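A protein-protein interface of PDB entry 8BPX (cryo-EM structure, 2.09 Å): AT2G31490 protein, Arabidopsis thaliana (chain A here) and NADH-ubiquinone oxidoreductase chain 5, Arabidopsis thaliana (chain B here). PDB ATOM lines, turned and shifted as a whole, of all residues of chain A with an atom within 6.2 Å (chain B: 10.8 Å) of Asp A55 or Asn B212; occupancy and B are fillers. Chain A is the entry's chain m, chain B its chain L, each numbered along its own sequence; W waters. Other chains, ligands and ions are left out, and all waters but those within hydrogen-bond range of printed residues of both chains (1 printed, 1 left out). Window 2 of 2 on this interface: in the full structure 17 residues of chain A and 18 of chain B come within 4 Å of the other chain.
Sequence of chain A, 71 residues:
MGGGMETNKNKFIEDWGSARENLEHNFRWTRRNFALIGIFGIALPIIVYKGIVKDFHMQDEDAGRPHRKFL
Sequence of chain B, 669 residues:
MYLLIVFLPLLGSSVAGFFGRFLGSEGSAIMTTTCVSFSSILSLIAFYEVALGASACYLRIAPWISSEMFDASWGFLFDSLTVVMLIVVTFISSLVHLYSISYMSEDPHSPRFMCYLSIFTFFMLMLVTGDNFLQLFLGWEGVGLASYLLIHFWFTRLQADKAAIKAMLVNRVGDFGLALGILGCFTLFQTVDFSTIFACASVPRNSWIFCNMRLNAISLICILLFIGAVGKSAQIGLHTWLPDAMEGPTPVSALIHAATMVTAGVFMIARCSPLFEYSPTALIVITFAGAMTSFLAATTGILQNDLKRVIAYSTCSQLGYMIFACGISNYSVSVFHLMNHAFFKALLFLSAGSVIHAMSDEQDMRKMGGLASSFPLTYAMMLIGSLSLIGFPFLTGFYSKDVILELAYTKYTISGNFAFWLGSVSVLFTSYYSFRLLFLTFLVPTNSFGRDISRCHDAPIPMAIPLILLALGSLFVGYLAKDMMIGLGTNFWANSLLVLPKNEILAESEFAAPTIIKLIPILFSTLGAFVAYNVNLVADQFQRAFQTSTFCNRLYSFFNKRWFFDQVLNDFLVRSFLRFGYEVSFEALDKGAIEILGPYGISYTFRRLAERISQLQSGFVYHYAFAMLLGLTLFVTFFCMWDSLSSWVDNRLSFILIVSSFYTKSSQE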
ATOM      1  N   LYS A  50       7.488   6.137  -6.589  1.00  0.00           N
ATOM      2  CA  LYS A  50       7.016   5.084  -5.625  1.00  0.00           C
ATOM      3  C   LYS A  50       8.228   4.456  -4.905  1.00  0.00           C
ATOM      4  O   LYS A  50       8.152   4.373  -3.712  1.00  0.00           O
ATOM      5  CB  LYS A  50       5.988   4.163  -6.293  1.00  0.00           C
ATOM      6  CG  LYS A  50       4.644   4.817  -6.544  1.00  0.00           C
ATOM      7  CD  LYS A  50       3.594   3.844  -6.993  1.00  0.00           C
ATOM      8  CE  LYS A  50       2.256   4.523  -7.171  1.00  0.00           C
ATOM      9  NZ  LYS A  50       1.827   5.204  -5.928  1.00  0.00           N
ATOM     10  N   GLY A  51       9.357   4.282  -5.581  1.00  0.00           N
ATOM     11  CA  GLY A  51      10.601   3.787  -4.969  1.00  0.00           C
ATOM     12  C   GLY A  51      11.160   4.712  -3.915  1.00  0.00           C
ATOM     13  O   GLY A  51      11.399   4.234  -2.845  1.00  0.00           O
ATOM     14  N   ILE A  52      11.238   6.007  -4.209  1.00  0.00           N
ATOM     15  CA  ILE A  52      11.788   7.044  -3.325  1.00  0.00           C
ATOM     16  C   ILE A  52      10.902   7.126  -2.093  1.00  0.00           C
ATOM     17  O   ILE A  52      11.475   7.174  -1.022  1.00  0.00           O
ATOM     18  CB  ILE A  52      12.025   8.384  -4.115  1.00  0.00           C
ATOM     19  CG1 ILE A  52      13.088   8.237  -5.205  1.00  0.00           C
ATOM     20  CG2 ILE A  52      12.302   9.552  -3.180  1.00  0.00           C
ATOM     21  CD1 ILE A  52      13.171   9.385  -6.167  1.00  0.00           C
ATOM     22  N   VAL A  53       9.588   7.084  -2.268  1.00  0.00           N
ATOM     23  CA  VAL A  53       8.622   7.243  -1.159  1.00  0.00           C
ATOM     24  C   VAL A  53       8.711   6.034  -0.221  1.00  0.00           C
ATOM     25  O   VAL A  53       8.763   6.233   0.938  1.00  0.00           O
ATOM     26  CB  VAL A  53       7.178   7.579  -1.634  1.00  0.00           C
ATOM     27  CG1 VAL A  53       6.120   7.365  -0.566  1.00  0.00           C
ATOM     28  CG2 VAL A  53       7.063   8.954  -2.269  1.00  0.00           C
ATOM     29  N   LYS A  54       8.768   4.865  -0.793  1.00  0.00           N
ATOM     30  CA  LYS A  54       8.869   3.607  -0.048  1.00  0.00           C
ATOM     31  C   LYS A  54      10.170   3.624   0.770  1.00  0.00           C
ATOM     32  O   LYS A  54      10.123   3.210   1.887  1.00  0.00           O
ATOM     33  CB  LYS A  54       8.726   2.454  -1.030  1.00  0.00           C
ATOM     34  CG  LYS A  54       9.301   1.126  -0.558  1.00  0.00           C
ATOM     35  CD  LYS A  54       8.812  -0.034  -1.385  1.00  0.00           C
ATOM     36  CE  LYS A  54       8.921  -1.364  -0.669  1.00  0.00           C
ATOM     37  NZ  LYS A  54      10.312  -1.872  -0.637  1.00  0.00           N
ATOM     38  N   ASP A  55      11.234   4.080   0.170  1.00  0.00           N
ATOM     39  CA  ASP A  55      12.526   4.208   0.862  1.00  0.00           C
ATOM     40  C   ASP A  55      12.313   5.033   2.138  1.00  0.00           C
ATOM     41  O   ASP A  55      12.589   4.463   3.202  1.00  0.00           O
ATOM     42  CB  ASP A  55      13.554   4.740  -0.123  1.00  0.00           C
ATOM     43  CG  ASP A  55      14.944   4.906   0.435  1.00  0.00           C
ATOM     44  OD1 ASP A  55      15.552   3.887   0.787  1.00  0.00           O
ATOM     45  OD2 ASP A  55      15.398   6.048   0.526  1.00  0.00           O
ATOM     46  N   PHE A  56      11.700   6.218   2.042  1.00  0.00           N
ATOM     47  CA  PHE A  56      11.386   7.001   3.248  1.00  0.00           C
ATOM     48  C   PHE A  56      10.471   6.214   4.235  1.00  0.00           C
ATOM     49  O   PHE A  56      10.663   6.402   5.414  1.00  0.00           O
ATOM     50  CB  PHE A  56      10.804   8.388   2.942  1.00  0.00           C
ATOM     51  CG  PHE A  56      11.712   9.417   2.309  1.00  0.00           C
ATOM     52  CD1 PHE A  56      12.804   9.932   2.991  1.00  0.00           C
ATOM     53  CD2 PHE A  56      11.427   9.937   1.059  1.00  0.00           C
ATOM     54  CE1 PHE A  56      13.603  10.914   2.429  1.00  0.00           C
ATOM     55  CE2 PHE A  56      12.229  10.916   0.488  1.00  0.00           C
ATOM     56  CZ  PHE A  56      13.312  11.411   1.176  1.00  0.00           C
ATOM     57  N   HIS A  57       9.479   5.477   3.759  1.00  0.00           N
ATOM     58  CA  HIS A  57       8.504   4.744   4.622  1.00  0.00           C
ATOM     59  C   HIS A  57       9.208   3.595   5.315  1.00  0.00           C
ATOM     60  O   HIS A  57       8.906   3.345   6.456  1.00  0.00           O
ATOM     61  CB  HIS A  57       7.290   4.278   3.783  1.00  0.00           C
ATOM     62  CG  HIS A  57       6.343   5.355   3.386  1.00  0.00           C
ATOM     63  ND1 HIS A  57       5.338   5.152   2.456  1.00  0.00           N
ATOM     64  CD2 HIS A  57       6.215   6.624   3.810  1.00  0.00           C
ATOM     65  CE1 HIS A  57       4.646   6.256   2.332  1.00  0.00           C
ATOM     66  NE2 HIS A  57       5.163   7.169   3.141  1.00  0.00           N
ATOM     67  N   MET A  58      10.115   2.964   4.601  1.00  0.00           N
ATOM     68  CA  MET A  58      10.899   1.875   5.187  1.00  0.00           C
ATOM     69  C   MET A  58      11.810   2.506   6.246  1.00  0.00           C
ATOM     70  O   MET A  58      11.919   1.890   7.293  1.00  0.00           O
ATOM     71  CB  MET A  58      11.586   1.000   4.130  1.00  0.00           C
ATOM     72  CG  MET A  58      10.681   0.093   3.357  1.00  0.00           C
ATOM     73  SD  MET A  58      11.569  -0.694   1.987  1.00  0.00           S
ATOM     74  CE  MET A  58      12.576  -1.904   2.841  1.00  0.00           C
ATOM     75  N   GLN A  59      12.390   3.672   6.017  1.00  0.00           N
ATOM     76  CA  GLN A  59      13.107   4.363   7.086  1.00  0.00           C
ATOM     77  C   GLN A  59      12.170   4.705   8.238  1.00  0.00           C
ATOM     78  O   GLN A  59      12.549   4.603   9.409  1.00  0.00           O
ATOM     79  CB  GLN A  59      13.767   5.633   6.557  1.00  0.00           C
ATOM     80  CG  GLN A  59      15.088   5.424   5.844  1.00  0.00           C
ATOM     81  CD  GLN A  59      15.641   6.723   5.284  1.00  0.00           C
ATOM     82  OE1 GLN A  59      16.546   7.322   5.860  1.00  0.00           O
ATOM     83  NE2 GLN A  59      15.086   7.172   4.167  1.00  0.00           N
ATOM     84  N   ASP A  60      10.941   5.120   7.922  1.00  0.00           N
ATOM     85  CA  ASP A  60       9.990   5.503   8.961  1.00  0.00           C
ATOM     86  C   ASP A  60       9.673   4.327   9.876  1.00  0.00           C
ATOM     87  O   ASP A  60       9.702   4.455  11.105  1.00  0.00           O
ATOM     88  CB  ASP A  60       8.709   6.039   8.326  1.00  0.00           C
ATOM     89  CG  ASP A  60       8.790   7.513   8.021  1.00  0.00           C
ATOM     90  OD1 ASP A  60       9.674   8.181   8.591  1.00  0.00           O
ATOM     91  OD2 ASP A  60       7.976   8.003   7.209  1.00  0.00           O
ATOM     92  N   SER B 207      20.876  -2.472  10.446  1.00  0.00           N
ATOM     93  CA  SER B 207      20.404  -2.752   9.103  1.00  0.00           C
ATOM     94  C   SER B 207      20.103  -1.447   8.383  1.00  0.00           C
ATOM     95  O   SER B 207      19.822  -0.422   9.007  1.00  0.00           O
ATOM     96  CB  SER B 207      19.157  -3.634   9.138  1.00  0.00           C
ATOM     97  OG  SER B 207      18.992  -4.332   7.919  1.00  0.00           O
ATOM     98  N   TRP B 208      20.158  -1.493   7.060  1.00  0.00           N
ATOM     99  CA  TRP B 208      19.994  -0.303   6.249  1.00  0.00           C
ATOM    100  C   TRP B 208      18.956  -0.556   5.169  1.00  0.00           C
ATOM    101  O   TRP B 208      18.709  -1.694   4.765  1.00  0.00           O
ATOM    102  CB  TRP B 208      21.315   0.120   5.615  1.00  0.00           C
ATOM    103  CG  TRP B 208      22.053   1.117   6.418  1.00  0.00           C
ATOM    104  CD1 TRP B 208      21.704   1.600   7.641  1.00  0.00           C
ATOM    105  CD2 TRP B 208      23.291   1.737   6.079  1.00  0.00           C
ATOM    106  NE1 TRP B 208      22.644   2.498   8.080  1.00  0.00           N
ATOM    107  CE2 TRP B 208      23.632   2.596   7.139  1.00  0.00           C
ATOM    108  CE3 TRP B 208      24.146   1.652   4.979  1.00  0.00           C
ATOM    109  CZ2 TRP B 208      24.791   3.367   7.130  1.00  0.00           C
ATOM    110  CZ3 TRP B 208      25.293   2.417   4.973  1.00  0.00           C
ATOM    111  CH2 TRP B 208      25.605   3.262   6.040  1.00  0.00           C
ATOM    112  N   ILE B 209      18.354   0.528   4.706  1.00  0.00           N
ATOM    113  CA  ILE B 209      17.431   0.494   3.584  1.00  0.00           C
ATOM    114  C   ILE B 209      18.218   0.901   2.347  1.00  0.00           C
ATOM    115  O   ILE B 209      18.591   2.068   2.191  1.00  0.00           O
ATOM    116  CB  ILE B 209      16.224   1.410   3.815  1.00  0.00           C
ATOM    117  CG1 ILE B 209      15.501   1.008   5.103  1.00  0.00           C
ATOM    118  CG2 ILE B 209      15.297   1.376   2.611  1.00  0.00           C
ATOM    119  CD1 ILE B 209      14.848  -0.355   5.047  1.00  0.00           C
ATOM    120  N   PHE B 210      18.492  -0.062   1.475  1.00  0.00           N
ATOM    121  CA  PHE B 210      19.202   0.192   0.228  1.00  0.00           C
ATOM    122  C   PHE B 210      18.344  -0.303  -0.925  1.00  0.00           C
ATOM    123  O   PHE B 210      18.113  -1.509  -1.056  1.00  0.00           O
ATOM    124  CB  PHE B 210      20.571  -0.480   0.210  1.00  0.00           C
ATOM    125  CG  PHE B 210      21.436  -0.021  -0.917  1.00  0.00           C
ATOM    126  CD1 PHE B 210      22.003   1.241  -0.900  1.00  0.00           C
ATOM    127  CD2 PHE B 210      21.648  -0.833  -2.017  1.00  0.00           C
ATOM    128  CE1 PHE B 210      22.790   1.674  -1.947  1.00  0.00           C
ATOM    129  CE2 PHE B 210      22.434  -0.404  -3.065  1.00  0.00           C
ATOM    130  CZ  PHE B 210      23.004   0.852  -3.032  1.00  0.00           C
ATOM    131  N   CYS B 211      17.902   0.630  -1.764  1.00  0.00           N
ATOM    132  CA  CYS B 211      17.025   0.331  -2.892  1.00  0.00           C
ATOM    133  C   CYS B 211      15.838  -0.520  -2.454  1.00  0.00           C
ATOM    134  O   CYS B 211      15.576  -1.600  -2.990  1.00  0.00           O
ATOM    135  CB  CYS B 211      17.802  -0.327  -4.029  1.00  0.00           C
ATOM    136  SG  CYS B 211      19.424   0.412  -4.302  1.00  0.00           S
ATOM    137  N   ASN B 212      15.147  -0.097  -1.411  1.00  0.00           N
ATOM    138  CA  ASN B 212      13.857  -0.678  -0.981  1.00  0.00           C
ATOM    139  C   ASN B 212      14.078  -2.082  -0.428  1.00  0.00           C
ATOM    140  O   ASN B 212      13.174  -2.858  -0.445  1.00  0.00           O
ATOM    141  CB  ASN B 212      12.767  -0.488  -2.050  1.00  0.00           C
ATOM    142  CG  ASN B 212      12.597   0.908  -2.611  1.00  0.00           C
ATOM    143  OD1 ASN B 212      12.017   1.064  -3.672  1.00  0.00           O
ATOM    144  ND2 ASN B 212      13.097   1.922  -1.938  1.00  0.00           N
ATOM    145  N   MET B 213      15.292  -2.319   0.030  1.00  0.00           N
ATOM    146  CA  MET B 213      15.622  -3.596   0.643  1.00  0.00           C
ATOM    147  C   MET B 213      16.294  -3.347   1.987  1.00  0.00           C
ATOM    148  O   MET B 213      17.000  -2.353   2.172  1.00  0.00           O
ATOM    149  CB  MET B 213      16.545  -4.434  -0.246  1.00  0.00           C
ATOM    150  CG  MET B 213      15.992  -4.732  -1.626  1.00  0.00           C
ATOM    151  SD  MET B 213      17.204  -5.495  -2.715  1.00  0.00           S
ATOM    152  CE  MET B 213      18.688  -4.599  -2.287  1.00  0.00           C
ATOM    153  N   ARG B 214      16.066  -4.257   2.923  1.00  0.00           N
ATOM    154  CA  ARG B 214      16.672  -4.191   4.246  1.00  0.00           C
ATOM    155  C   ARG B 214      17.901  -5.091   4.247  1.00  0.00           C
ATOM    156  O   ARG B 214      17.780  -6.308   4.083  1.00  0.00           O
ATOM    157  CB  ARG B 214      15.676  -4.621   5.319  1.00  0.00           C
ATOM    158  CG  ARG B 214      15.587  -3.682   6.502  1.00  0.00           C
ATOM    159  CD  ARG B 214      14.298  -3.892   7.278  1.00  0.00           C
ATOM    160  NE  ARG B 214      13.120  -3.838   6.423  1.00  0.00           N
ATOM    161  CZ  ARG B 214      12.228  -2.856   6.428  1.00  0.00           C
ATOM    162  NH1 ARG B 214      12.357  -1.810   7.224  1.00  0.00           N
ATOM    163  NH2 ARG B 214      11.182  -2.925   5.613  1.00  0.00           N
ATOM    164  N   LEU B 215      19.077  -4.492   4.413  1.00  0.00           N
ATOM    165  CA  LEU B 215      20.343  -5.210   4.340  1.00  0.00           C
ATOM    166  C   LEU B 215      21.235  -4.820   5.511  1.00  0.00           C
ATOM    167  O   LEU B 215      21.041  -3.785   6.151  1.00  0.00           O
ATOM    168  CB  LEU B 215      21.082  -4.932   3.018  1.00  0.00           C
ATOM    169  CG  LEU B 215      20.317  -4.619   1.728  1.00  0.00           C
ATOM    170  CD1 LEU B 215      21.281  -4.310   0.597  1.00  0.00           C
ATOM    171  CD2 LEU B 215      19.423  -5.776   1.331  1.00  0.00           C
ATOM    172  N   LEU B 220      26.705  -4.345   2.996  1.00  0.00           N
ATOM    173  CA  LEU B 220      26.424  -3.489   1.850  1.00  0.00           C
ATOM    174  C   LEU B 220      27.643  -2.657   1.486  1.00  0.00           C
ATOM    175  O   LEU B 220      28.030  -2.575   0.313  1.00  0.00           O
ATOM    176  CB  LEU B 220      25.227  -2.589   2.163  1.00  0.00           C
ATOM    177  CG  LEU B 220      24.960  -1.406   1.229  1.00  0.00           C
ATOM    178  CD1 LEU B 220      24.597  -1.897  -0.154  1.00  0.00           C
ATOM    179  CD2 LEU B 220      23.864  -0.521   1.793  1.00  0.00           C
HETATM  180  O   HOH W   1      17.340   4.495   2.334  1.00  0.00           O
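The backbone carbonyl oxygen of Gly A51 is in hydrogen-bond range of the side-chain amide nitrogen of Asn B212 (3.0 Å). The side-chain amino group (NZ) of Lys A54 sits at hydrogen-bond distance from the backbone carbonyl oxygen (O) of Asn B212 (3.0 Å). SD of Met A58 sits close to O of Asn B212, 3.6 Å away.
NZ of Lys A54 sits at hydrogen-bond distance from SD of Met A58 (3.1 Å).
Among the printed residues, merely in contact across the chains: Asp A55 with Ile B209, Met A58 with Arg B214, Asp A55 with Asn B212, Met A58 with Ile B209 and Met A58 with Met B213.
Gly A51 touches just one residue of chain B: Asn B212. Asp A55 touches just these residues of chain B: Ile B209 (3.1 Å) and Asn B212 (3.4 Å). No residue of chain B comes within 4 Å of Gln A59. Ser B207 touches none of the printed residues of chain A. Printed residues of chain A within 4 Å of Ile B209: Asp A55 and Met A58. Asn B212 touches just these residues of chain A: Gly A51, Lys A54, Asp A55 and Met A58. Of the printed residues of chain A, Met B213 touches Met A58. Of the printed residues of chain A, Arg B214 touches Met A58.
Printed residues of chain B that touch a printed residue of chain A: Ile B209, Asn B212, Met B213 and Arg B214. Hydrophobic or aromatic side chains of chain A that line the printed part of chain B: Met A58. Among the printed residues, no Asp or Glu carboxylate lies within 4 Å of a Lys or Arg side-chain nitrogen of the other chain.
Water W1 bridges the side-chain carboxylate (OD1) of Asp A55 (2.4 Å) and the backbone carbonyl oxygen (O) of Ile B209 (2.7 Å).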
